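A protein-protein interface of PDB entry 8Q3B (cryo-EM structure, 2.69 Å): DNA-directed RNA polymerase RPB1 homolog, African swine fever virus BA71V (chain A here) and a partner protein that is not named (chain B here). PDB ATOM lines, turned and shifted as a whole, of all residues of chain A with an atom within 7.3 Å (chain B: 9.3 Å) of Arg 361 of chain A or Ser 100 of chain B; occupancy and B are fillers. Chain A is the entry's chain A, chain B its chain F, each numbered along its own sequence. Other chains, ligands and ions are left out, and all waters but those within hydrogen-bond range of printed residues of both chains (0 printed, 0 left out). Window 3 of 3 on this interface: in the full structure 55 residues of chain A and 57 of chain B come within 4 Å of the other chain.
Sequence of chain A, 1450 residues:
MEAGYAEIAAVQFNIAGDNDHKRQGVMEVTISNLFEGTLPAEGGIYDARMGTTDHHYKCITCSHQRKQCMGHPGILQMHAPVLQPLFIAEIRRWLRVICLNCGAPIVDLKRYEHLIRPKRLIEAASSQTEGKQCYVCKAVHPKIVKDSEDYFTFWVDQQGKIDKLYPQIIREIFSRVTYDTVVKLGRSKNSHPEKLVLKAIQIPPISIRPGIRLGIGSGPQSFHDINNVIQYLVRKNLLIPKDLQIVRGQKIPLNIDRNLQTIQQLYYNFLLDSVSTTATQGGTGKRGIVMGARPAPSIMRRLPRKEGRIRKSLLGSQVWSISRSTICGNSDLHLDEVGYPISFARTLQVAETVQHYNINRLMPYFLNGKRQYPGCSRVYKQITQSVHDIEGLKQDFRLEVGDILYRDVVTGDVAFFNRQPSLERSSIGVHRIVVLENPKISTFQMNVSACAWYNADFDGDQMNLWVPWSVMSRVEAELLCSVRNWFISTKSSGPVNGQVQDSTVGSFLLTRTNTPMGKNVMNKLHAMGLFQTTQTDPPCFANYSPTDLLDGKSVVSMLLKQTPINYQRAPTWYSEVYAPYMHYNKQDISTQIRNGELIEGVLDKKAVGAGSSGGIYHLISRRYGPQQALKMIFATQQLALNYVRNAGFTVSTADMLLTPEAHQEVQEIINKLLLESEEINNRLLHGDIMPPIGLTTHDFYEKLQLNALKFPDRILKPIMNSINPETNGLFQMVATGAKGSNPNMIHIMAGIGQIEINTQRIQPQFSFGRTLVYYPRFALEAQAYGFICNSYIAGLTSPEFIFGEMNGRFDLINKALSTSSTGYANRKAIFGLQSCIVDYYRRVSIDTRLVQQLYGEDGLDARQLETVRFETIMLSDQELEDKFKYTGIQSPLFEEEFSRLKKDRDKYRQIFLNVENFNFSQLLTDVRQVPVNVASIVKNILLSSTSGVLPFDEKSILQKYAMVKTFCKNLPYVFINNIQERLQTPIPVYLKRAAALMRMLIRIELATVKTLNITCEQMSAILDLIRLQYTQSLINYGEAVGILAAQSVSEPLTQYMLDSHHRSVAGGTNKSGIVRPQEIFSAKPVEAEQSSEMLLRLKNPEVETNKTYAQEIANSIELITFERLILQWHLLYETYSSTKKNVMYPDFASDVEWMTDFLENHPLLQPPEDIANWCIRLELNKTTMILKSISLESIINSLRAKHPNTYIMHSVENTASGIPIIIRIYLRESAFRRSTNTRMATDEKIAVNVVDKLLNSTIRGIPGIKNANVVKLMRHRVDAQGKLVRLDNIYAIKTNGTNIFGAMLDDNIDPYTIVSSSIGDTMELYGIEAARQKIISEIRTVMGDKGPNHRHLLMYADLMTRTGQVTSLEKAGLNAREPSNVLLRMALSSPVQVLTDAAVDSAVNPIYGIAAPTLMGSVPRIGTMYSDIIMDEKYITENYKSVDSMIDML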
ATOM      1  N   GLU A 352     -16.789 -23.503  17.030  1.00  0.00           N
ATOM      2  CA  GLU A 352     -16.154 -24.601  16.313  1.00  0.00           C
ATOM      3  C   GLU A 352     -16.762 -25.908  16.795  1.00  0.00           C
ATOM      4  O   GLU A 352     -16.772 -26.181  17.999  1.00  0.00           O
ATOM      5  CB  GLU A 352     -14.640 -24.602  16.537  1.00  0.00           C
ATOM      6  CG  GLU A 352     -13.954 -23.302  16.155  1.00  0.00           C
ATOM      7  CD  GLU A 352     -13.092 -23.441  14.917  1.00  0.00           C
ATOM      8  OE1 GLU A 352     -13.559 -24.048  13.931  1.00  0.00           O
ATOM      9  OE2 GLU A 352     -11.948 -22.942  14.930  1.00  0.00           O
ATOM     10  N   THR A 353     -17.268 -26.711  15.863  1.00  0.00           N
ATOM     11  CA  THR A 353     -17.844 -28.004  16.207  1.00  0.00           C
ATOM     12  C   THR A 353     -16.725 -29.032  16.319  1.00  0.00           C
ATOM     13  O   THR A 353     -16.022 -29.303  15.341  1.00  0.00           O
ATOM     14  CB  THR A 353     -18.869 -28.432  15.160  1.00  0.00           C
ATOM     15  OG1 THR A 353     -19.846 -27.398  14.994  1.00  0.00           O
ATOM     16  CG2 THR A 353     -19.568 -29.713  15.589  1.00  0.00           C
ATOM     17  N   TYR A 357     -10.864 -34.099  13.549  1.00  0.00           N
ATOM     18  CA  TYR A 357      -9.801 -33.282  12.980  1.00  0.00           C
ATOM     19  C   TYR A 357      -9.599 -31.963  13.716  1.00  0.00           C
ATOM     20  O   TYR A 357      -8.548 -31.335  13.547  1.00  0.00           O
ATOM     21  CB  TYR A 357     -10.082 -32.991  11.498  1.00  0.00           C
ATOM     22  CG  TYR A 357     -11.481 -32.495  11.206  1.00  0.00           C
ATOM     23  CD1 TYR A 357     -12.527 -33.385  11.003  1.00  0.00           C
ATOM     24  CD2 TYR A 357     -11.755 -31.139  11.134  1.00  0.00           C
ATOM     25  CE1 TYR A 357     -13.804 -32.934  10.737  1.00  0.00           C
ATOM     26  CE2 TYR A 357     -13.030 -30.681  10.871  1.00  0.00           C
ATOM     27  CZ  TYR A 357     -14.050 -31.582  10.674  1.00  0.00           C
ATOM     28  OH  TYR A 357     -15.319 -31.127  10.410  1.00  0.00           O
ATOM     29  N   ASN A 358     -10.567 -31.531  14.523  1.00  0.00           N
ATOM     30  CA  ASN A 358     -10.442 -30.296  15.285  1.00  0.00           C
ATOM     31  C   ASN A 358      -9.905 -30.506  16.693  1.00  0.00           C
ATOM     32  O   ASN A 358      -9.477 -29.534  17.325  1.00  0.00           O
ATOM     33  CB  ASN A 358     -11.801 -29.596  15.392  1.00  0.00           C
ATOM     34  CG  ASN A 358     -12.294 -29.068  14.067  1.00  0.00           C
ATOM     35  OD1 ASN A 358     -11.561 -29.053  13.082  1.00  0.00           O
ATOM     36  ND2 ASN A 358     -13.545 -28.627  14.036  1.00  0.00           N
ATOM     37  N   ILE A 359      -9.916 -31.740  17.198  1.00  0.00           N
ATOM     38  CA  ILE A 359      -9.644 -31.962  18.616  1.00  0.00           C
ATOM     39  C   ILE A 359      -8.244 -31.475  18.975  1.00  0.00           C
ATOM     40  O   ILE A 359      -8.052 -30.760  19.965  1.00  0.00           O
ATOM     41  CB  ILE A 359      -9.845 -33.447  18.973  1.00  0.00           C
ATOM     42  CG1 ILE A 359      -9.727 -33.663  20.484  1.00  0.00           C
ATOM     43  CG2 ILE A 359      -8.847 -34.327  18.233  1.00  0.00           C
ATOM     44  CD1 ILE A 359     -10.831 -33.008  21.285  1.00  0.00           C
ATOM     45  N   ASN A 360      -7.246 -31.843  18.170  1.00  0.00           N
ATOM     46  CA  ASN A 360      -5.878 -31.434  18.470  1.00  0.00           C
ATOM     47  C   ASN A 360      -5.717 -29.923  18.379  1.00  0.00           C
ATOM     48  O   ASN A 360      -5.062 -29.311  19.229  1.00  0.00           O
ATOM     49  CB  ASN A 360      -4.902 -32.136  17.528  1.00  0.00           C
ATOM     50  CG  ASN A 360      -4.733 -33.605  17.853  1.00  0.00           C
ATOM     51  OD1 ASN A 360      -5.292 -34.104  18.829  1.00  0.00           O
ATOM     52  ND2 ASN A 360      -3.956 -34.306  17.037  1.00  0.00           N
ATOM     53  N   ARG A 361      -6.305 -29.304  17.354  1.00  0.00           N
ATOM     54  CA  ARG A 361      -6.188 -27.858  17.205  1.00  0.00           C
ATOM     55  C   ARG A 361      -6.994 -27.113  18.262  1.00  0.00           C
ATOM     56  O   ARG A 361      -6.579 -26.038  18.708  1.00  0.00           O
ATOM     57  CB  ARG A 361      -6.639 -27.433  15.809  1.00  0.00           C
ATOM     58  CG  ARG A 361      -6.591 -25.931  15.579  1.00  0.00           C
ATOM     59  CD  ARG A 361      -6.873 -25.576  14.133  1.00  0.00           C
ATOM     60  NE  ARG A 361      -8.204 -26.000  13.715  1.00  0.00           N
ATOM     61  CZ  ARG A 361      -9.328 -25.383  14.052  1.00  0.00           C
ATOM     62  NH1 ARG A 361      -9.323 -24.305  14.819  1.00  0.00           N
ATOM     63  NH2 ARG A 361     -10.487 -25.859  13.608  1.00  0.00           N
ATOM     64  N   LEU A 362      -8.144 -27.655  18.663  1.00  0.00           N
ATOM     65  CA  LEU A 362      -9.004 -26.966  19.618  1.00  0.00           C
ATOM     66  C   LEU A 362      -8.602 -27.207  21.066  1.00  0.00           C
ATOM     67  O   LEU A 362      -9.065 -26.477  21.948  1.00  0.00           O
ATOM     68  CB  LEU A 362     -10.459 -27.398  19.423  1.00  0.00           C
ATOM     69  CG  LEU A 362     -11.151 -26.965  18.130  1.00  0.00           C
ATOM     70  CD1 LEU A 362     -12.589 -27.450  18.127  1.00  0.00           C
ATOM     71  CD2 LEU A 362     -11.099 -25.457  17.945  1.00  0.00           C
ATOM     72  N   MET A 363      -7.762 -28.205  21.337  1.00  0.00           N
ATOM     73  CA  MET A 363      -7.393 -28.489  22.722  1.00  0.00           C
ATOM     74  C   MET A 363      -6.698 -27.311  23.389  1.00  0.00           C
ATOM     75  O   MET A 363      -7.034 -27.001  24.546  1.00  0.00           O
ATOM     76  CB  MET A 363      -6.516 -29.745  22.774  1.00  0.00           C
ATOM     77  CG  MET A 363      -7.210 -31.037  23.238  1.00  0.00           C
ATOM     78  SD  MET A 363      -8.586 -30.860  24.397  1.00  0.00           S
ATOM     79  CE  MET A 363      -7.713 -30.771  25.957  1.00  0.00           C
ATOM     80  N   PRO A 364      -5.726 -26.640  22.764  1.00  0.00           N
ATOM     81  CA  PRO A 364      -5.126 -25.467  23.422  1.00  0.00           C
ATOM     82  C   PRO A 364      -6.140 -24.396  23.782  1.00  0.00           C
ATOM     83  O   PRO A 364      -6.037 -23.787  24.854  1.00  0.00           O
ATOM     84  CB  PRO A 364      -4.112 -24.970  22.382  1.00  0.00           C
ATOM     85  CG  PRO A 364      -3.782 -26.171  21.572  1.00  0.00           C
ATOM     86  CD  PRO A 364      -5.038 -26.986  21.511  1.00  0.00           C
ATOM     87  N   TYR A 365      -7.128 -24.154  22.917  1.00  0.00           N
ATOM     88  CA  TYR A 365      -8.168 -23.181  23.237  1.00  0.00           C
ATOM     89  C   TYR A 365      -8.927 -23.597  24.489  1.00  0.00           C
ATOM     90  O   TYR A 365      -9.194 -22.776  25.373  1.00  0.00           O
ATOM     91  CB  TYR A 365      -9.133 -23.039  22.060  1.00  0.00           C
ATOM     92  CG  TYR A 365      -8.525 -22.444  20.812  1.00  0.00           C
ATOM     93  CD1 TYR A 365      -8.435 -21.070  20.647  1.00  0.00           C
ATOM     94  CD2 TYR A 365      -8.049 -23.256  19.794  1.00  0.00           C
ATOM     95  CE1 TYR A 365      -7.887 -20.524  19.504  1.00  0.00           C
ATOM     96  CE2 TYR A 365      -7.498 -22.719  18.650  1.00  0.00           C
ATOM     97  CZ  TYR A 365      -7.419 -21.352  18.511  1.00  0.00           C
ATOM     98  OH  TYR A 365      -6.870 -20.811  17.372  1.00  0.00           O
ATOM     99  N   PHE A 366      -9.286 -24.879  24.578  1.00  0.00           N
ATOM    100  CA  PHE A 366     -10.026 -25.367  25.735  1.00  0.00           C
ATOM    101  C   PHE A 366      -9.196 -25.257  27.007  1.00  0.00           C
ATOM    102  O   PHE A 366      -9.703 -24.842  28.056  1.00  0.00           O
ATOM    103  CB  PHE A 366     -10.455 -26.812  25.493  1.00  0.00           C
ATOM    104  CG  PHE A 366     -11.223 -27.417  26.629  1.00  0.00           C
ATOM    105  CD1 PHE A 366     -12.563 -27.122  26.810  1.00  0.00           C
ATOM    106  CD2 PHE A 366     -10.609 -28.287  27.510  1.00  0.00           C
ATOM    107  CE1 PHE A 366     -13.269 -27.680  27.852  1.00  0.00           C
ATOM    108  CE2 PHE A 366     -11.312 -28.847  28.553  1.00  0.00           C
ATOM    109  CZ  PHE A 366     -12.644 -28.543  28.723  1.00  0.00           C
ATOM    110  N   LEU A 405     -17.306 -25.582  20.779  1.00  0.00           N
ATOM    111  CA  LEU A 405     -16.418 -24.755  21.581  1.00  0.00           C
ATOM    112  C   LEU A 405     -16.456 -23.330  21.050  1.00  0.00           C
ATOM    113  O   LEU A 405     -16.260 -23.108  19.851  1.00  0.00           O
ATOM    114  CB  LEU A 405     -14.990 -25.302  21.536  1.00  0.00           C
ATOM    115  CG  LEU A 405     -13.919 -24.513  22.291  1.00  0.00           C
ATOM    116  CD1 LEU A 405     -14.070 -24.704  23.787  1.00  0.00           C
ATOM    117  CD2 LEU A 405     -12.534 -24.931  21.832  1.00  0.00           C
ATOM    118  N   ARG A 407     -14.514 -20.270  20.916  1.00  0.00           N
ATOM    119  CA  ARG A 407     -13.149 -19.809  21.114  1.00  0.00           C
ATOM    120  C   ARG A 407     -13.028 -18.329  20.770  1.00  0.00           C
ATOM    121  O   ARG A 407     -13.907 -17.732  20.147  1.00  0.00           O
ATOM    122  CB  ARG A 407     -12.178 -20.637  20.268  1.00  0.00           C
ATOM    123  CG  ARG A 407     -12.508 -20.670  18.786  1.00  0.00           C
ATOM    124  CD  ARG A 407     -11.284 -21.010  17.957  1.00  0.00           C
ATOM    125  NE  ARG A 407     -11.511 -20.817  16.531  1.00  0.00           N
ATOM    126  CZ  ARG A 407     -11.346 -19.667  15.891  1.00  0.00           C
ATOM    127  NH1 ARG A 407     -10.965 -18.570  16.523  1.00  0.00           N
ATOM    128  NH2 ARG A 407     -11.569 -19.618  14.581  1.00  0.00           N
ATOM    129  N   VAL A 410      -8.945 -14.994  16.624  1.00  0.00           N
ATOM    130  CA  VAL A 410      -7.500 -15.037  16.463  1.00  0.00           C
ATOM    131  C   VAL A 410      -7.138 -14.441  15.110  1.00  0.00           C
ATOM    132  O   VAL A 410      -7.985 -14.268  14.230  1.00  0.00           O
ATOM    133  CB  VAL A 410      -6.943 -16.469  16.590  1.00  0.00           C
ATOM    134  CG1 VAL A 410      -7.195 -17.010  17.985  1.00  0.00           C
ATOM    135  CG2 VAL A 410      -7.562 -17.380  15.542  1.00  0.00           C
ATOM    136  N   ARG A 474     -19.124 -17.903   7.790  1.00  0.00           N
ATOM    137  CA  ARG A 474     -17.689 -17.712   7.609  1.00  0.00           C
ATOM    138  C   ARG A 474     -17.268 -18.044   6.184  1.00  0.00           C
ATOM    139  O   ARG A 474     -16.491 -17.303   5.566  1.00  0.00           O
ATOM    140  CB  ARG A 474     -16.917 -18.576   8.605  1.00  0.00           C
ATOM    141  CG  ARG A 474     -16.968 -18.070  10.031  1.00  0.00           C
ATOM    142  CD  ARG A 474     -16.633 -19.172  11.015  1.00  0.00           C
ATOM    143  NE  ARG A 474     -15.320 -19.751  10.760  1.00  0.00           N
ATOM    144  CZ  ARG A 474     -14.904 -20.911  11.247  1.00  0.00           C
ATOM    145  NH1 ARG A 474     -15.678 -21.654  12.023  1.00  0.00           N
ATOM    146  NH2 ARG A 474     -13.682 -21.340  10.949  1.00  0.00           N
ATOM    147  N   THR B  93     -14.871 -37.740   5.182  1.00  0.00           N
ATOM    148  CA  THR B  93     -14.505 -37.020   3.972  1.00  0.00           C
ATOM    149  C   THR B  93     -13.754 -37.946   3.027  1.00  0.00           C
ATOM    150  O   THR B  93     -13.034 -38.851   3.459  1.00  0.00           O
ATOM    151  CB  THR B  93     -13.633 -35.794   4.282  1.00  0.00           C
ATOM    152  OG1 THR B  93     -13.034 -35.313   3.074  1.00  0.00           O
ATOM    153  CG2 THR B  93     -12.539 -36.150   5.277  1.00  0.00           C
ATOM    154  N   LYS B  97      -5.825 -36.071   1.624  1.00  0.00           N
ATOM    155  CA  LYS B  97      -5.072 -35.182   2.494  1.00  0.00           C
ATOM    156  C   LYS B  97      -5.898 -34.819   3.724  1.00  0.00           C
ATOM    157  O   LYS B  97      -7.131 -34.842   3.711  1.00  0.00           O
ATOM    158  CB  LYS B  97      -4.661 -33.917   1.742  1.00  0.00           C
ATOM    159  CG  LYS B  97      -3.622 -33.084   2.472  1.00  0.00           C
ATOM    160  CD  LYS B  97      -3.129 -31.930   1.619  1.00  0.00           C
ATOM    161  CE  LYS B  97      -2.271 -30.974   2.430  1.00  0.00           C
ATOM    162  NZ  LYS B  97      -1.903 -29.755   1.659  1.00  0.00           N
ATOM    163  N   LYS B  98      -5.196 -34.478   4.801  1.00  0.00           N
ATOM    164  CA  LYS B  98      -5.811 -34.197   6.091  1.00  0.00           C
ATOM    165  C   LYS B  98      -5.767 -32.702   6.375  1.00  0.00           C
ATOM    166  O   LYS B  98      -4.707 -32.076   6.269  1.00  0.00           O
ATOM    167  CB  LYS B  98      -5.103 -34.965   7.208  1.00  0.00           C
ATOM    168  CG  LYS B  98      -5.814 -36.242   7.624  1.00  0.00           C
ATOM    169  CD  LYS B  98      -5.758 -37.293   6.528  1.00  0.00           C
ATOM    170  CE  LYS B  98      -6.704 -38.447   6.818  1.00  0.00           C
ATOM    171  NZ  LYS B  98      -8.096 -38.150   6.378  1.00  0.00           N
ATOM    172  N   TYR B  99      -6.918 -32.140   6.734  1.00  0.00           N
ATOM    173  CA  TYR B  99      -7.031 -30.749   7.139  1.00  0.00           C
ATOM    174  C   TYR B  99      -7.727 -30.679   8.490  1.00  0.00           C
ATOM    175  O   TYR B  99      -8.469 -31.585   8.877  1.00  0.00           O
ATOM    176  CB  TYR B  99      -7.802 -29.915   6.108  1.00  0.00           C
ATOM    177  CG  TYR B  99      -7.104 -29.784   4.776  1.00  0.00           C
ATOM    178  CD1 TYR B  99      -7.293 -30.726   3.775  1.00  0.00           C
ATOM    179  CD2 TYR B  99      -6.256 -28.717   4.520  1.00  0.00           C
ATOM    180  CE1 TYR B  99      -6.656 -30.608   2.557  1.00  0.00           C
ATOM    181  CE2 TYR B  99      -5.614 -28.592   3.306  1.00  0.00           C
ATOM    182  CZ  TYR B  99      -5.816 -29.540   2.328  1.00  0.00           C
ATOM    183  OH  TYR B  99      -5.180 -29.416   1.116  1.00  0.00           O
ATOM    184  N   SER B 100      -7.473 -29.589   9.208  1.00  0.00           N
ATOM    185  CA  SER B 100      -7.979 -29.405  10.560  1.00  0.00           C
ATOM    186  C   SER B 100      -9.172 -28.461  10.628  1.00  0.00           C
ATOM    187  O   SER B 100      -9.582 -28.082  11.728  1.00  0.00           O
ATOM    188  CB  SER B 100      -6.860 -28.890  11.467  1.00  0.00           C
ATOM    189  OG  SER B 100      -6.959 -27.490  11.647  1.00  0.00           O
ATOM    190  N   SER B 101      -9.734 -28.065   9.485  1.00  0.00           N
ATOM    191  CA  SER B 101     -10.882 -27.172   9.460  1.00  0.00           C
ATOM    192  C   SER B 101     -11.885 -27.653   8.420  1.00  0.00           C
ATOM    193  O   SER B 101     -11.485 -28.067   7.322  1.00  0.00           O
ATOM    194  CB  SER B 101     -10.465 -25.731   9.142  1.00  0.00           C
ATOM    195  OG  SER B 101     -11.593 -24.927   8.851  1.00  0.00           O
ATOM    196  N   PRO B 102     -13.185 -27.614   8.728  1.00  0.00           N
ATOM    197  CA  PRO B 102     -14.175 -28.030   7.722  1.00  0.00           C
ATOM    198  C   PRO B 102     -14.171 -27.161   6.479  1.00  0.00           C
ATOM    199  O   PRO B 102     -14.434 -27.663   5.380  1.00  0.00           O
ATOM    200  CB  PRO B 102     -15.505 -27.929   8.481  1.00  0.00           C
ATOM    201  CG  PRO B 102     -15.257 -26.929   9.545  1.00  0.00           C
ATOM    202  CD  PRO B 102     -13.826 -27.101   9.950  1.00  0.00           C
ATOM    203  N   ILE B 103     -13.880 -25.866   6.620  1.00  0.00           N
ATOM    204  CA  ILE B 103     -13.889 -24.972   5.466  1.00  0.00           C
ATOM    205  C   ILE B 103     -12.827 -25.392   4.461  1.00  0.00           C
ATOM    206  O   ILE B 103     -13.080 -25.438   3.251  1.00  0.00           O
ATOM    207  CB  ILE B 103     -13.694 -23.515   5.922  1.00  0.00           C
ATOM    208  CG1 ILE B 103     -14.823 -23.116   6.879  1.00  0.00           C
ATOM    209  CG2 ILE B 103     -13.620 -22.588   4.710  1.00  0.00           C
ATOM    210  CD1 ILE B 103     -14.801 -21.666   7.313  1.00  0.00           C
ATOM    211  N   ASP B 104     -11.619 -25.694   4.940  1.00  0.00           N
ATOM    212  CA  ASP B 104     -10.555 -26.120   4.037  1.00  0.00           C
ATOM    213  C   ASP B 104     -10.902 -27.441   3.365  1.00  0.00           C
ATOM    214  O   ASP B 104     -10.644 -27.625   2.170  1.00  0.00           O
ATOM    215  CB  ASP B 104      -9.239 -26.235   4.800  1.00  0.00           C
ATOM    216  CG  ASP B 104      -8.614 -24.887   5.088  1.00  0.00           C
ATOM    217  OD1 ASP B 104      -8.452 -24.091   4.139  1.00  0.00           O
ATOM    218  OD2 ASP B 104      -8.286 -24.621   6.263  1.00  0.00           O
ATOM    219  N   ILE B 105     -11.485 -28.375   4.119  1.00  0.00           N
ATOM    220  CA  ILE B 105     -11.871 -29.659   3.541  1.00  0.00           C
ATOM    221  C   ILE B 105     -12.893 -29.449   2.432  1.00  0.00           C
ATOM    222  O   ILE B 105     -12.789 -30.037   1.352  1.00  0.00           O
ATOM    223  CB  ILE B 105     -12.409 -30.601   4.634  1.00  0.00           C
ATOM    224  CG1 ILE B 105     -11.335 -30.860   5.691  1.00  0.00           C
ATOM    225  CG2 ILE B 105     -12.869 -31.918   4.022  1.00  0.00           C
ATOM    226  CD1 ILE B 105     -11.846 -31.568   6.926  1.00  0.00           C
ATOM    227  N   ALA B 106     -13.898 -28.606   2.683  1.00  0.00           N
ATOM    228  CA  ALA B 106     -14.916 -28.355   1.667  1.00  0.00           C
ATOM    229  C   ALA B 106     -14.323 -27.663   0.445  1.00  0.00           C
ATOM    230  O   ALA B 106     -14.668 -27.999  -0.695  1.00  0.00           O
ATOM    231  CB  ALA B 106     -16.047 -27.516   2.259  1.00  0.00           C
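The backbone carbonyl oxygen (O) of Ser 100 of chain B lies close to the side-chain amide oxygen (OD1) of Asn 358 of chain A (2.6 Å).
OG of Ser 100 of chain B is in hydrogen-bond range of NE of Arg 361 of chain A, 2.8 Å away.
The side-chain carboxylate (OE2) of Glu 352 of chain A is in salt-bridge range of the guanidinium group (NH1) of Arg 361 of chain A, at 3.0 Å.
OE1 of Glu 352 of chain A is in salt-bridge range of NH1 of Arg 474 of chain A, 3.7 Å away.
O of Thr 353 of chain A lies within hydrogen-bond range of ND2 of Asn 358 of chain A (2.9 Å).
The side-chain amide oxygen (OD1) of Asn 358 of chain A is in hydrogen-bond range of the guanidinium group (NH2) of Arg 361 of chain A (3.4 Å).
The side-chain hydroxyl (OH) of Tyr 99 of chain B lies close to the side-chain amino group (NZ) of Lys 97 of chain B (3.3 Å).
OG of Ser 101 of chain B sits close to N of Ile 103 of chain B (3.3 Å).
Among the printed residues, merely in contact across the chains: Tyr 357 of chain A with Tyr 99 of chain B, Tyr 357 of chain A with Ser 100 of chain B, Tyr 357 of chain A with Pro 102 of chain B and Arg 474 of chain A with Ile 103 of chain B.
Glu 352 of chain A touches none of the printed residues of chain B.
Of the printed residues of chain B, Tyr 357 of chain A touches Tyr 99, Ser 100 and Pro 102.
Of chain B, only Ser 100 (2.6 Å) comes within 4 Å of Asn 358 of chain A.
Arg 361 of chain A touches just one residue of chain B: Ser 100.
Of the printed residues of chain B, Arg 474 of chain A touches Ile 103.
Of the printed residues of chain A, Tyr 99 of chain B touches Tyr 357 (3.4 Å).
Of the printed residues of chain A, Pro 102 of chain B touches Tyr 357.
Of the printed residues of chain A, Ile 103 of chain B touches Arg 474 (3.8 Å).
The nearest residue of chain B that does not touch Arg 361 of chain A is Ser 101 of chain B (4.4 Å).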
